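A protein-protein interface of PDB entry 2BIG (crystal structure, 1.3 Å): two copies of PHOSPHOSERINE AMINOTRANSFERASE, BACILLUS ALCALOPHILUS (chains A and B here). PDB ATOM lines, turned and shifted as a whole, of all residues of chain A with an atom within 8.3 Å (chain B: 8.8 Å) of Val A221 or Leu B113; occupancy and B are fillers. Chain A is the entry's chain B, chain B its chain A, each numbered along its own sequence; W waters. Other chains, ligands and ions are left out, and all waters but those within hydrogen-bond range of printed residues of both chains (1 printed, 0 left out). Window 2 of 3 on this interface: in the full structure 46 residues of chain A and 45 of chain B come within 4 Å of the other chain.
The side-chain carboxylate (OE2) of Glu B110 lies within hydrogen-bond range of the side-chain hydroxyl (OG1) of Thr A223 (2.6 Å).
OG1 of Thr A229 sits at hydrogen-bond distance from O of Thr A223 (2.7 Å).
ND2 of Asn A87 is in hydrogen-bond range of O of Leu A225 (2.8 Å).
O of Val A221 lies within hydrogen-bond range of NE2 of Gln A226 (2.8 Å).
Val A221 touches Leu B113.
Pro A222 touches Thr B82 (CG to OG1, 3.2 Å).
Pro A222 touches Met B86.
Pro A222 touches Glu B110 (CA to OE1, 3.7 Å).
CA of Pro A222 touches CD1 of Leu B113, at 3.95 Å.
CD1 of Leu A225 touches CE of Met B86, 3.8 Å away.
CD1 of Leu B225 touches CD1 of Leu A225, at 3.8 Å.
Val A221 touches just one residue of chain B: Leu B113.
Of the printed residues of chain B, Leu A225 touches Met B86 (3.8 Å) and Leu B225 (3.8 Å).
Ala A228 touches none of the printed residues of chain B.
Of the printed residues of chain A, Met B86 touches Pro A222 (3.6 Å) and Leu A225 (3.8 Å).
Lys B109 touches none of the printed residues of chain A.
Printed residues of chain A within 4 Å of Leu B225: Leu A225 (3.8 Å).
The nearest residue of chain A that does not touch Leu B113 is Thr A223 (4.3 Å).
The nearest printed residue of chain B that does not touch Pro A222 is Leu B114 (4.6 Å).
Of the 19 printed residues of chain A, 4 touch a printed residue of chain B.
Printed residues of chain A that touch a printed residue of chain B: Val A221, Pro A222, Thr A223 and Leu A225.
Of the 19 printed residues of chain B, 5 touch a printed residue of chain A.
Among the printed residues, 8 pairs touch across the chains.
Leu A225 touches Met B86, but with the chains exchanged Met A86 does not touch Leu B225 (4.2 Å).
Leu B225 touches its own counterpart, Leu A225.
4 positions are printed for both chains.
Water W1 lies within hydrogen-bond range of the backbone NH (N) of Met A224 (2.8 Å), the side-chain carboxylate (OE1) of Glu B110 (2.9 Å) and the backbone NH (N) of Thr A223 (3.3 Å).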
ATOM      1  N   THR A  82       6.944  10.893  -9.710  1.00  0.00           N
ATOM      2  CA  THR A  82       5.708  10.414 -10.322  1.00  0.00           C
ATOM      3  C   THR A  82       4.482  10.600  -9.434  1.00  0.00           C
ATOM      4  O   THR A  82       3.405  10.905  -9.960  1.00  0.00           O
ATOM      5  CB  THR A  82       5.889   8.959 -10.794  1.00  0.00           C
ATOM      6  OG1 THR A  82       4.725   8.616 -11.591  1.00  0.00           O
ATOM      7  CG2 THR A  82       5.902   7.952  -9.687  1.00  0.00           C
ATOM      8  N   MET A  83       4.612  10.431  -8.113  1.00  0.00           N
ATOM      9  CA  MET A  83       3.430  10.511  -7.253  1.00  0.00           C
ATOM     10  C   MET A  83       2.810  11.903  -7.333  1.00  0.00           C
ATOM     11  O   MET A  83       1.567  12.044  -7.289  1.00  0.00           O
ATOM     12  CB  MET A  83       3.813  10.140  -5.824  1.00  0.00           C
ATOM     13  CG  MET A  83       2.661   9.825  -4.929  1.00  0.00           C
ATOM     14  SD  MET A  83       3.267   9.069  -3.393  1.00  0.00           S
ATOM     15  CE  MET A  83       1.791   9.172  -2.401  1.00  0.00           C
ATOM     16  N   PRO A  85       2.663  14.269  -9.909  1.00  0.00           N
ATOM     17  CA  PRO A  85       1.747  14.457 -11.068  1.00  0.00           C
ATOM     18  C   PRO A  85       0.622  13.446 -11.025  1.00  0.00           C
ATOM     19  O   PRO A  85      -0.467  13.756 -11.475  1.00  0.00           O
ATOM     20  CB  PRO A  85       2.641  14.326 -12.312  1.00  0.00           C
ATOM     21  CG  PRO A  85       3.856  13.564 -11.806  1.00  0.00           C
ATOM     22  CD  PRO A  85       4.040  14.049 -10.412  1.00  0.00           C
ATOM     23  N   MET A  86       0.852  12.268 -10.487  1.00  0.00           N
ATOM     24  CA  MET A  86      -0.238  11.310 -10.446  1.00  0.00           C
ATOM     25  C   MET A  86      -1.434  11.849  -9.647  1.00  0.00           C
ATOM     26  O   MET A  86      -2.573  11.479  -9.949  1.00  0.00           O
ATOM     27  CB  MET A  86       0.281  10.004  -9.863  1.00  0.00           C
ATOM     28  CG  MET A  86      -0.553   8.812 -10.258  1.00  0.00           C
ATOM     29  SD  MET A  86       0.132   7.251  -9.694  1.00  0.00           S
ATOM     30  CE  MET A  86       1.518   6.960 -10.802  1.00  0.00           C
ATOM     31  N   ASN A  87      -1.159  12.636  -8.643  1.00  0.00           N
ATOM     32  CA  ASN A  87      -2.211  13.189  -7.797  1.00  0.00           C
ATOM     33  C   ASN A  87      -2.686  14.537  -8.266  1.00  0.00           C
ATOM     34  O   ASN A  87      -3.871  14.826  -8.103  1.00  0.00           O
ATOM     35  CB  ASN A  87      -1.746  13.302  -6.359  1.00  0.00           C
ATOM     36  CG  ASN A  87      -1.733  12.004  -5.597  1.00  0.00           C
ATOM     37  OD1 ASN A  87      -2.610  11.761  -4.758  1.00  0.00           O
ATOM     38  ND2 ASN A  87      -0.749  11.160  -5.865  1.00  0.00           N
ATOM     39  N   LEU A  88      -1.830  15.380  -8.837  1.00  0.00           N
ATOM     40  CA  LEU A  88      -2.236  16.762  -9.074  1.00  0.00           C
ATOM     41  C   LEU A  88      -2.323  17.118 -10.551  1.00  0.00           C
ATOM     42  O   LEU A  88      -2.949  18.138 -10.863  1.00  0.00           O
ATOM     43  CB  LEU A  88      -1.200  17.652  -8.369  1.00  0.00           C
ATOM     44  CG  LEU A  88      -1.524  19.096  -8.062  1.00  0.00           C
ATOM     45  CD1 LEU A  88      -2.906  19.208  -7.439  1.00  0.00           C
ATOM     46  CD2 LEU A  88      -0.476  19.695  -7.136  1.00  0.00           C
ATOM     47  N   THR A  90      -4.008  16.858 -13.389  1.00  0.00           N
ATOM     48  CA  THR A  90      -5.292  16.334 -13.843  1.00  0.00           C
ATOM     49  C   THR A  90      -5.557  16.842 -15.253  1.00  0.00           C
ATOM     50  O   THR A  90      -4.872  17.725 -15.792  1.00  0.00           O
ATOM     51  CB  THR A  90      -6.321  16.786 -12.796  1.00  0.00           C
ATOM     52  OG1 THR A  90      -6.334  18.226 -12.782  1.00  0.00           O
ATOM     53  CG2 THR A  90      -5.879  16.335 -11.410  1.00  0.00           C
ATOM     54  N   VAL A 218      -8.801  11.129  -5.622  1.00  0.00           N
ATOM     55  CA  VAL A 218      -8.159  10.964  -6.952  1.00  0.00           C
ATOM     56  C   VAL A 218      -8.404   9.501  -7.367  1.00  0.00           C
ATOM     57  O   VAL A 218      -7.681   8.526  -7.240  1.00  0.00           O
ATOM     58  CB  VAL A 218      -6.723  11.505  -6.975  1.00  0.00           C
ATOM     59  CG1 VAL A 218      -5.708  10.582  -6.364  1.00  0.00           C
ATOM     60  CG2 VAL A 218      -6.374  11.861  -8.422  1.00  0.00           C
ATOM     61  N   GLU A 219      -9.639   9.384  -7.870  1.00  0.00           N
ATOM     62  CA  GLU A 219     -10.260   8.311  -8.576  1.00  0.00           C
ATOM     63  C   GLU A 219      -9.150   7.728  -9.479  1.00  0.00           C
ATOM     64  O   GLU A 219      -8.432   8.509 -10.139  1.00  0.00           O
ATOM     65  CB  GLU A 219     -11.541   8.800  -9.276  1.00  0.00           C
ATOM     66  N   GLN A 220      -9.050   6.403  -9.367  1.00  0.00           N
ATOM     67  CA  GLN A 220      -8.233   5.633 -10.271  1.00  0.00           C
ATOM     68  C   GLN A 220      -6.764   5.574  -9.883  1.00  0.00           C
ATOM     69  O   GLN A 220      -6.033   4.824 -10.532  1.00  0.00           O
ATOM     70  CB  GLN A 220      -8.299   6.187 -11.695  1.00  0.00           C
ATOM     71  CG  GLN A 220      -9.304   5.482 -12.599  1.00  0.00           C
ATOM     72  CD  GLN A 220      -9.112   5.971 -14.030  1.00  0.00           C
ATOM     73  OE1 GLN A 220      -8.952   5.184 -14.952  1.00  0.00           O
ATOM     74  NE2 GLN A 220      -9.118   7.294 -14.177  1.00  0.00           N
ATOM     75  N   VAL A 221      -6.339   6.329  -8.865  1.00  0.00           N
ATOM     76  CA  VAL A 221      -4.942   6.212  -8.430  1.00  0.00           C
ATOM     77  C   VAL A 221      -4.808   5.079  -7.439  1.00  0.00           C
ATOM     78  O   VAL A 221      -5.614   4.989  -6.492  1.00  0.00           O
ATOM     79  CB  VAL A 221      -4.474   7.568  -7.846  1.00  0.00           C
ATOM     80  CG1 VAL A 221      -3.045   7.494  -7.318  1.00  0.00           C
ATOM     81  CG2 VAL A 221      -4.599   8.657  -8.912  1.00  0.00           C
ATOM     82  N   PRO A 222      -3.834   4.204  -7.612  1.00  0.00           N
ATOM     83  CA  PRO A 222      -3.621   3.141  -6.619  1.00  0.00           C
ATOM     84  C   PRO A 222      -3.530   3.675  -5.213  1.00  0.00           C
ATOM     85  O   PRO A 222      -2.974   4.733  -4.964  1.00  0.00           O
ATOM     86  CB  PRO A 222      -2.301   2.555  -7.088  1.00  0.00           C
ATOM     87  CG  PRO A 222      -2.294   2.717  -8.564  1.00  0.00           C
ATOM     88  CD  PRO A 222      -2.924   4.073  -8.762  1.00  0.00           C
ATOM     89  N   THR A 223      -4.066   2.899  -4.259  1.00  0.00           N
ATOM     90  CA  THR A 223      -4.163   3.308  -2.874  1.00  0.00           C
ATOM     91  C   THR A 223      -2.836   3.813  -2.337  1.00  0.00           C
ATOM     92  O   THR A 223      -2.790   4.895  -1.700  1.00  0.00           O
ATOM     93  CB  THR A 223      -4.665   2.110  -2.045  1.00  0.00           C
ATOM     94  OG1 THR A 223      -5.891   1.642  -2.614  1.00  0.00           O
ATOM     95  CG2 THR A 223      -4.910   2.584  -0.616  1.00  0.00           C
ATOM     96  N   MET A 224      -1.749   3.096  -2.536  1.00  0.00           N
ATOM     97  CA  MET A 224      -0.446   3.506  -1.967  1.00  0.00           C
ATOM     98  C   MET A 224       0.094   4.775  -2.602  1.00  0.00           C
ATOM     99  O   MET A 224       0.991   5.392  -2.019  1.00  0.00           O
ATOM    100  CB  MET A 224       0.569   2.374  -2.170  1.00  0.00           C
ATOM    101  CG  MET A 224       0.547   1.280  -1.107  1.00  0.00           C
ATOM    102  SD  MET A 224       0.966   1.853   0.552  1.00  0.00           S
ATOM    103  CE  MET A 224       2.721   2.143   0.366  1.00  0.00           C
ATOM    104  N   LEU A 225      -0.413   5.149  -3.761  1.00  0.00           N
ATOM    105  CA  LEU A 225       0.104   6.296  -4.523  1.00  0.00           C
ATOM    106  C   LEU A 225      -0.769   7.503  -4.380  1.00  0.00           C
ATOM    107  O   LEU A 225      -0.438   8.511  -4.978  1.00  0.00           O
ATOM    108  CB  LEU A 225       0.311   5.884  -5.998  1.00  0.00           C
ATOM    109  CG  LEU A 225       1.427   4.845  -6.188  1.00  0.00           C
ATOM    110  CD1 LEU A 225       1.399   4.221  -7.574  1.00  0.00           C
ATOM    111  CD2 LEU A 225       2.783   5.492  -5.907  1.00  0.00           C
ATOM    112  N   GLN A 226      -1.808   7.445  -3.579  1.00  0.00           N
ATOM    113  CA  GLN A 226      -2.592   8.637  -3.209  1.00  0.00           C
ATOM    114  C   GLN A 226      -2.012   9.315  -1.984  1.00  0.00           C
ATOM    115  O   GLN A 226      -1.860   8.663  -0.933  1.00  0.00           O
ATOM    116  CB  GLN A 226      -4.032   8.242  -2.863  1.00  0.00           C
ATOM    117  CG  GLN A 226      -4.790   7.712  -4.054  1.00  0.00           C
ATOM    118  CD  GLN A 226      -6.261   7.549  -3.744  1.00  0.00           C
ATOM    119  OE1 GLN A 226      -6.873   8.304  -2.981  1.00  0.00           O
ATOM    120  NE2 GLN A 226      -6.757   6.510  -4.372  1.00  0.00           N
ATOM    121  N   TYR A 227      -1.741  10.627  -2.026  1.00  0.00           N
ATOM    122  CA  TYR A 227      -1.416  11.321  -0.784  1.00  0.00           C
ATOM    123  C   TYR A 227      -2.527  11.154   0.229  1.00  0.00           C
ATOM    124  O   TYR A 227      -2.214  11.031   1.421  1.00  0.00           O
ATOM    125  CB  TYR A 227      -1.098  12.804  -1.031  1.00  0.00           C
ATOM    126  CG  TYR A 227       0.179  12.952  -1.824  1.00  0.00           C
ATOM    127  CD1 TYR A 227       0.110  13.328  -3.143  1.00  0.00           C
ATOM    128  CD2 TYR A 227       1.446  12.705  -1.307  1.00  0.00           C
ATOM    129  CE1 TYR A 227       1.242  13.467  -3.910  1.00  0.00           C
ATOM    130  CE2 TYR A 227       2.582  12.841  -2.082  1.00  0.00           C
ATOM    131  CZ  TYR A 227       2.482  13.231  -3.374  1.00  0.00           C
ATOM    132  OH  TYR A 227       3.605  13.364  -4.157  1.00  0.00           O
ATOM    133  N   ALA A 228      -3.777  11.153  -0.209  1.00  0.00           N
ATOM    134  CA  ALA A 228      -4.874  11.053   0.730  1.00  0.00           C
ATOM    135  C   ALA A 228      -4.778   9.851   1.639  1.00  0.00           C
ATOM    136  O   ALA A 228      -5.156   9.917   2.808  1.00  0.00           O
ATOM    137  CB  ALA A 228      -6.202  11.011  -0.077  1.00  0.00           C
ATOM    138  N   THR A 229      -4.350   8.729   1.096  1.00  0.00           N
ATOM    139  CA  THR A 229      -4.204   7.508   1.896  1.00  0.00           C
ATOM    140  C   THR A 229      -3.313   7.735   3.097  1.00  0.00           C
ATOM    141  O   THR A 229      -3.620   7.367   4.216  1.00  0.00           O
ATOM    142  CB  THR A 229      -3.570   6.426   1.016  1.00  0.00           C
ATOM    143  OG1 THR A 229      -4.498   6.140  -0.030  1.00  0.00           O
ATOM    144  CG2 THR A 229      -3.266   5.133   1.760  1.00  0.00           C
ATOM    145  N   PHE B  81       1.242  -4.842  -4.383  1.00  0.00           N
ATOM    146  CA  PHE B  81      -0.145  -5.135  -4.766  1.00  0.00           C
ATOM    147  C   PHE B  81      -0.522  -4.339  -6.003  1.00  0.00           C
ATOM    148  O   PHE B  81      -1.303  -4.825  -6.813  1.00  0.00           O
ATOM    149  CB  PHE B  81      -1.126  -4.804  -3.664  1.00  0.00           C
ATOM    150  CG  PHE B  81      -1.014  -5.570  -2.356  1.00  0.00           C
ATOM    151  CD1 PHE B  81      -1.582  -5.078  -1.199  1.00  0.00           C
ATOM    152  CD2 PHE B  81      -0.361  -6.796  -2.293  1.00  0.00           C
ATOM    153  CE1 PHE B  81      -1.564  -5.765   0.006  1.00  0.00           C
ATOM    154  CE2 PHE B  81      -0.334  -7.509  -1.108  1.00  0.00           C
ATOM    155  CZ  PHE B  81      -0.924  -7.004  -0.009  1.00  0.00           C
ATOM    156  N   THR B  82      -0.013  -3.136  -6.162  1.00  0.00           N
ATOM    157  CA  THR B  82      -0.274  -2.344  -7.387  1.00  0.00           C
ATOM    158  C   THR B  82       0.805  -2.508  -8.445  1.00  0.00           C
ATOM    159  O   THR B  82       0.498  -2.597  -9.667  1.00  0.00           O
ATOM    160  CB  THR B  82      -0.542  -0.853  -7.029  1.00  0.00           C
ATOM    161  OG1 THR B  82      -1.064  -0.233  -8.241  1.00  0.00           O
ATOM    162  CG2 THR B  82       0.657  -0.048  -6.652  1.00  0.00           C
ATOM    163  N   PRO B  85       0.091  -5.775 -10.935  1.00  0.00           N
ATOM    164  CA  PRO B  85      -0.848  -5.578 -12.057  1.00  0.00           C
ATOM    165  C   PRO B  85      -0.442  -4.442 -12.981  1.00  0.00           C
ATOM    166  O   PRO B  85      -0.675  -4.499 -14.185  1.00  0.00           O
ATOM    167  CB  PRO B  85      -2.199  -5.329 -11.384  1.00  0.00           C
ATOM    168  CG  PRO B  85      -1.851  -4.878  -9.996  1.00  0.00           C
ATOM    169  CD  PRO B  85      -0.609  -5.646  -9.658  1.00  0.00           C
ATOM    170  N   MET B  86       0.231  -3.431 -12.455  1.00  0.00           N
ATOM    171  CA  MET B  86       0.688  -2.372 -13.367  1.00  0.00           C
ATOM    172  C   MET B  86       1.616  -2.902 -14.446  1.00  0.00           C
ATOM    173  O   MET B  86       1.655  -2.411 -15.575  1.00  0.00           O
ATOM    174  CB  MET B  86       1.527  -1.342 -12.609  1.00  0.00           C
ATOM    175  CG  MET B  86       0.705  -0.262 -11.980  1.00  0.00           C
ATOM    176  SD  MET B  86       1.819   0.955 -11.290  1.00  0.00           S
ATOM    177  CE  MET B  86       0.622   2.080 -10.592  1.00  0.00           C
ATOM    178  N   LEU B  89      -0.776  -6.906 -15.812  1.00  0.00           N
ATOM    179  CA  LEU B  89      -2.216  -6.967 -16.129  1.00  0.00           C
ATOM    180  C   LEU B  89      -2.501  -6.094 -17.320  1.00  0.00           C
ATOM    181  O   LEU B  89      -2.861  -4.913 -17.229  1.00  0.00           O
ATOM    182  CB  LEU B  89      -3.033  -6.566 -14.911  1.00  0.00           C
ATOM    183  CG  LEU B  89      -4.539  -6.703 -15.040  1.00  0.00           C
ATOM    184  CD1 LEU B  89      -4.934  -8.077 -15.575  1.00  0.00           C
ATOM    185  CD2 LEU B  89      -5.166  -6.400 -13.701  1.00  0.00           C
ATOM    186  N   TYR B  97      -7.070 -14.225  -8.653  1.00  0.00           N
ATOM    187  CA  TYR B  97      -6.668 -14.248  -7.244  1.00  0.00           C
ATOM    188  C   TYR B  97      -7.289 -15.411  -6.493  1.00  0.00           C
ATOM    189  O   TYR B  97      -8.474 -15.703  -6.695  1.00  0.00           O
ATOM    190  CB  TYR B  97      -7.085 -12.923  -6.525  1.00  0.00           C
ATOM    191  CG  TYR B  97      -6.141 -11.802  -6.987  1.00  0.00           C
ATOM    192  CD1 TYR B  97      -6.277 -11.243  -8.231  1.00  0.00           C
ATOM    193  CD2 TYR B  97      -5.105 -11.357  -6.169  1.00  0.00           C
ATOM    194  CE1 TYR B  97      -5.416 -10.249  -8.648  1.00  0.00           C
ATOM    195  CE2 TYR B  97      -4.220 -10.373  -6.581  1.00  0.00           C
ATOM    196  CZ  TYR B  97      -4.395  -9.800  -7.837  1.00  0.00           C
ATOM    197  OH  TYR B  97      -3.517  -8.836  -8.289  1.00  0.00           O
ATOM    198  N   LYS B 106      -6.724  -7.431  -0.097  1.00  0.00           N
ATOM    199  CA  LYS B 106      -6.079  -6.149  -0.360  1.00  0.00           C
ATOM    200  C   LYS B 106      -5.339  -6.211  -1.703  1.00  0.00           C
ATOM    201  O   LYS B 106      -5.283  -5.216  -2.456  1.00  0.00           O
ATOM    202  CB  LYS B 106      -5.169  -5.771   0.795  1.00  0.00           C
ATOM    203  CG  LYS B 106      -5.947  -5.444   2.071  1.00  0.00           C
ATOM    204  CD  LYS B 106      -5.279  -4.358   2.830  1.00  0.00           C
ATOM    205  CE  LYS B 106      -5.812  -4.091   4.225  1.00  0.00           C
ATOM    206  NZ  LYS B 106      -4.857  -3.179   4.948  1.00  0.00           N
ATOM    207  N   ALA B 107      -4.737  -7.355  -2.017  1.00  0.00           N
ATOM    208  CA  ALA B 107      -4.049  -7.484  -3.297  1.00  0.00           C
ATOM    209  C   ALA B 107      -5.037  -7.436  -4.466  1.00  0.00           C
ATOM    210  O   ALA B 107      -4.828  -6.748  -5.475  1.00  0.00           O
ATOM    211  CB  ALA B 107      -3.253  -8.781  -3.321  1.00  0.00           C
ATOM    212  N   LEU B 108      -6.119  -8.150  -4.322  1.00  0.00           N
ATOM    213  CA  LEU B 108      -7.163  -8.126  -5.363  1.00  0.00           C
ATOM    214  C   LEU B 108      -7.684  -6.733  -5.611  1.00  0.00           C
ATOM    215  O   LEU B 108      -7.888  -6.322  -6.766  1.00  0.00           O
ATOM    216  CB  LEU B 108      -8.297  -9.050  -4.930  1.00  0.00           C
ATOM    217  CG  LEU B 108      -9.589  -8.989  -5.748  1.00  0.00           C
ATOM    218  CD1 LEU B 108      -9.372  -9.448  -7.180  1.00  0.00           C
ATOM    219  CD2 LEU B 108     -10.681  -9.790  -5.091  1.00  0.00           C
ATOM    220  N   LYS B 109      -7.963  -5.978  -4.526  1.00  0.00           N
ATOM    221  CA  LYS B 109      -8.521  -4.621  -4.645  1.00  0.00           C
ATOM    222  C   LYS B 109      -7.639  -3.763  -5.541  1.00  0.00           C
ATOM    223  O   LYS B 109      -8.128  -3.003  -6.376  1.00  0.00           O
ATOM    224  CB  LYS B 109      -8.667  -3.992  -3.248  1.00  0.00           C
ATOM    225  CG  LYS B 109      -9.020  -2.510  -3.260  1.00  0.00           C
ATOM    226  CD  LYS B 109      -9.012  -1.978  -1.817  1.00  0.00           C
ATOM    227  CE  LYS B 109      -9.224  -0.467  -1.703  1.00  0.00           C
ATOM    228  NZ  LYS B 109      -9.347  -0.113  -0.261  1.00  0.00           N
ATOM    229  N   GLU B 110      -6.307  -3.827  -5.394  1.00  0.00           N
ATOM    230  CA  GLU B 110      -5.444  -3.005  -6.218  1.00  0.00           C
ATOM    231  C   GLU B 110      -5.494  -3.397  -7.684  1.00  0.00           C
ATOM    232  O   GLU B 110      -5.431  -2.516  -8.551  1.00  0.00           O
ATOM    233  CB  GLU B 110      -4.005  -3.029  -5.682  1.00  0.00           C
ATOM    234  CG  GLU B 110      -3.900  -2.392  -4.304  1.00  0.00           C
ATOM    235  CD  GLU B 110      -4.543  -1.021  -4.173  1.00  0.00           C
ATOM    236  OE1 GLU B 110      -4.207  -0.139  -5.011  1.00  0.00           O
ATOM    237  OE2 GLU B 110      -5.356  -0.835  -3.233  1.00  0.00           O
ATOM    238  N   ALA B 111      -5.598  -4.689  -7.973  1.00  0.00           N
ATOM    239  CA  ALA B 111      -5.701  -5.123  -9.349  1.00  0.00           C
ATOM    240  C   ALA B 111      -7.000  -4.641 -10.002  1.00  0.00           C
ATOM    241  O   ALA B 111      -6.991  -4.285 -11.184  1.00  0.00           O
ATOM    242  CB  ALA B 111      -5.538  -6.632  -9.473  1.00  0.00           C
ATOM    243  N   LYS B 112      -8.068  -4.576  -9.220  1.00  0.00           N
ATOM    244  CA  LYS B 112      -9.347  -4.124  -9.733  1.00  0.00           C
ATOM    245  C   LYS B 112      -9.287  -2.699 -10.239  1.00  0.00           C
ATOM    246  O   LYS B 112     -10.060  -2.358 -11.136  1.00  0.00           O
ATOM    247  CB  LYS B 112     -10.425  -4.180  -8.644  1.00  0.00           C
ATOM    248  CG  LYS B 112     -10.898  -5.580  -8.371  1.00  0.00           C
ATOM    249  CD  LYS B 112     -12.159  -5.634  -7.501  1.00  0.00           C
ATOM    250  CE  LYS B 112     -12.665  -7.047  -7.302  1.00  0.00           C
ATOM    251  NZ  LYS B 112     -13.707  -7.119  -6.235  1.00  0.00           N
ATOM    252  N   LEU B 113      -8.401  -1.910  -9.699  1.00  0.00           N
ATOM    253  CA  LEU B 113      -8.260  -0.545 -10.148  1.00  0.00           C
ATOM    254  C   LEU B 113      -7.563  -0.498 -11.495  1.00  0.00           C
ATOM    255  O   LEU B 113      -7.617   0.562 -12.137  1.00  0.00           O
ATOM    256  CB  LEU B 113      -7.423   0.315  -9.178  1.00  0.00           C
ATOM    257  CG  LEU B 113      -8.075   0.582  -7.824  1.00  0.00           C
ATOM    258  CD1 LEU B 113      -7.130   1.335  -6.860  1.00  0.00           C
ATOM    259  CD2 LEU B 113      -9.385   1.351  -8.019  1.00  0.00           C
ATOM    260  N   LEU B 114      -6.930  -1.581 -11.893  1.00  0.00           N
ATOM    261  CA  LEU B 114      -6.131  -1.492 -13.094  1.00  0.00           C
ATOM    262  C   LEU B 114      -6.579  -2.358 -14.242  1.00  0.00           C
ATOM    263  O   LEU B 114      -6.131  -2.163 -15.390  1.00  0.00           O
ATOM    264  CB  LEU B 114      -4.669  -1.805 -12.733  1.00  0.00           C
ATOM    265  CG  LEU B 114      -4.041  -0.821 -11.747  1.00  0.00           C
ATOM    266  CD1 LEU B 114      -2.701  -1.378 -11.243  1.00  0.00           C
ATOM    267  CD2 LEU B 114      -3.761   0.539 -12.339  1.00  0.00           C
ATOM    268  N   GLY B 115      -7.438  -3.307 -14.014  1.00  0.00           N
ATOM    269  CA  GLY B 115      -7.876  -4.170 -15.101  1.00  0.00           C
ATOM    270  C   GLY B 115      -8.865  -5.191 -14.583  1.00  0.00           C
ATOM    271  O   GLY B 115      -9.387  -5.093 -13.476  1.00  0.00           O
ATOM    272  N   GLU B 116      -9.106  -6.158 -15.462  1.00  0.00           N
ATOM    273  CA  GLU B 116     -10.071  -7.216 -15.156  1.00  0.00           C
ATOM    274  C   GLU B 116      -9.459  -8.181 -14.144  1.00  0.00           C
ATOM    275  O   GLU B 116      -8.285  -8.518 -14.207  1.00  0.00           O
ATOM    276  CB  GLU B 116     -10.399  -8.019 -16.425  1.00  0.00           C
ATOM    277  CG  GLU B 116     -11.536  -8.986 -16.149  1.00  0.00           C
ATOM    278  CD  GLU B 116     -12.262  -9.566 -17.329  1.00  0.00           C
ATOM    279  OE1 GLU B 116     -11.868  -9.355 -18.507  1.00  0.00           O
ATOM    280  OE2 GLU B 116     -13.268 -10.253 -17.003  1.00  0.00           O
ATOM    281  N   THR B 117     -10.251  -8.645 -13.204  1.00  0.00           N
ATOM    282  CA  THR B 117      -9.879  -9.522 -12.138  1.00  0.00           C
ATOM    283  C   THR B 117     -10.878 -10.677 -12.067  1.00  0.00           C
ATOM    284  O   THR B 117     -11.961 -10.658 -12.629  1.00  0.00           O
ATOM    285  CB  THR B 117      -9.814  -8.870 -10.752  1.00  0.00           C
ATOM    286  OG1 THR B 117     -11.080  -8.305 -10.382  1.00  0.00           O
ATOM    287  CG2 THR B 117      -8.796  -7.745 -10.745  1.00  0.00           C
ATOM    288  N   LEU B 225       8.067   2.464 -11.154  1.00  0.00           N
ATOM    289  CA  LEU B 225       7.089   1.421 -10.980  1.00  0.00           C
ATOM    290  C   LEU B 225       7.215   0.304 -11.987  1.00  0.00           C
ATOM    291  O   LEU B 225       6.407  -0.625 -11.980  1.00  0.00           O
ATOM    292  CB  LEU B 225       5.648   2.017 -11.003  1.00  0.00           C
ATOM    293  CG  LEU B 225       5.372   2.938  -9.813  1.00  0.00           C
ATOM    294  CD1 LEU B 225       4.173   3.798 -10.123  1.00  0.00           C
ATOM    295  CD2 LEU B 225       5.217   2.107  -8.562  1.00  0.00           C
HETATM  296  O   HOH W   1      -1.675   0.647  -3.963  1.00  0.00           O
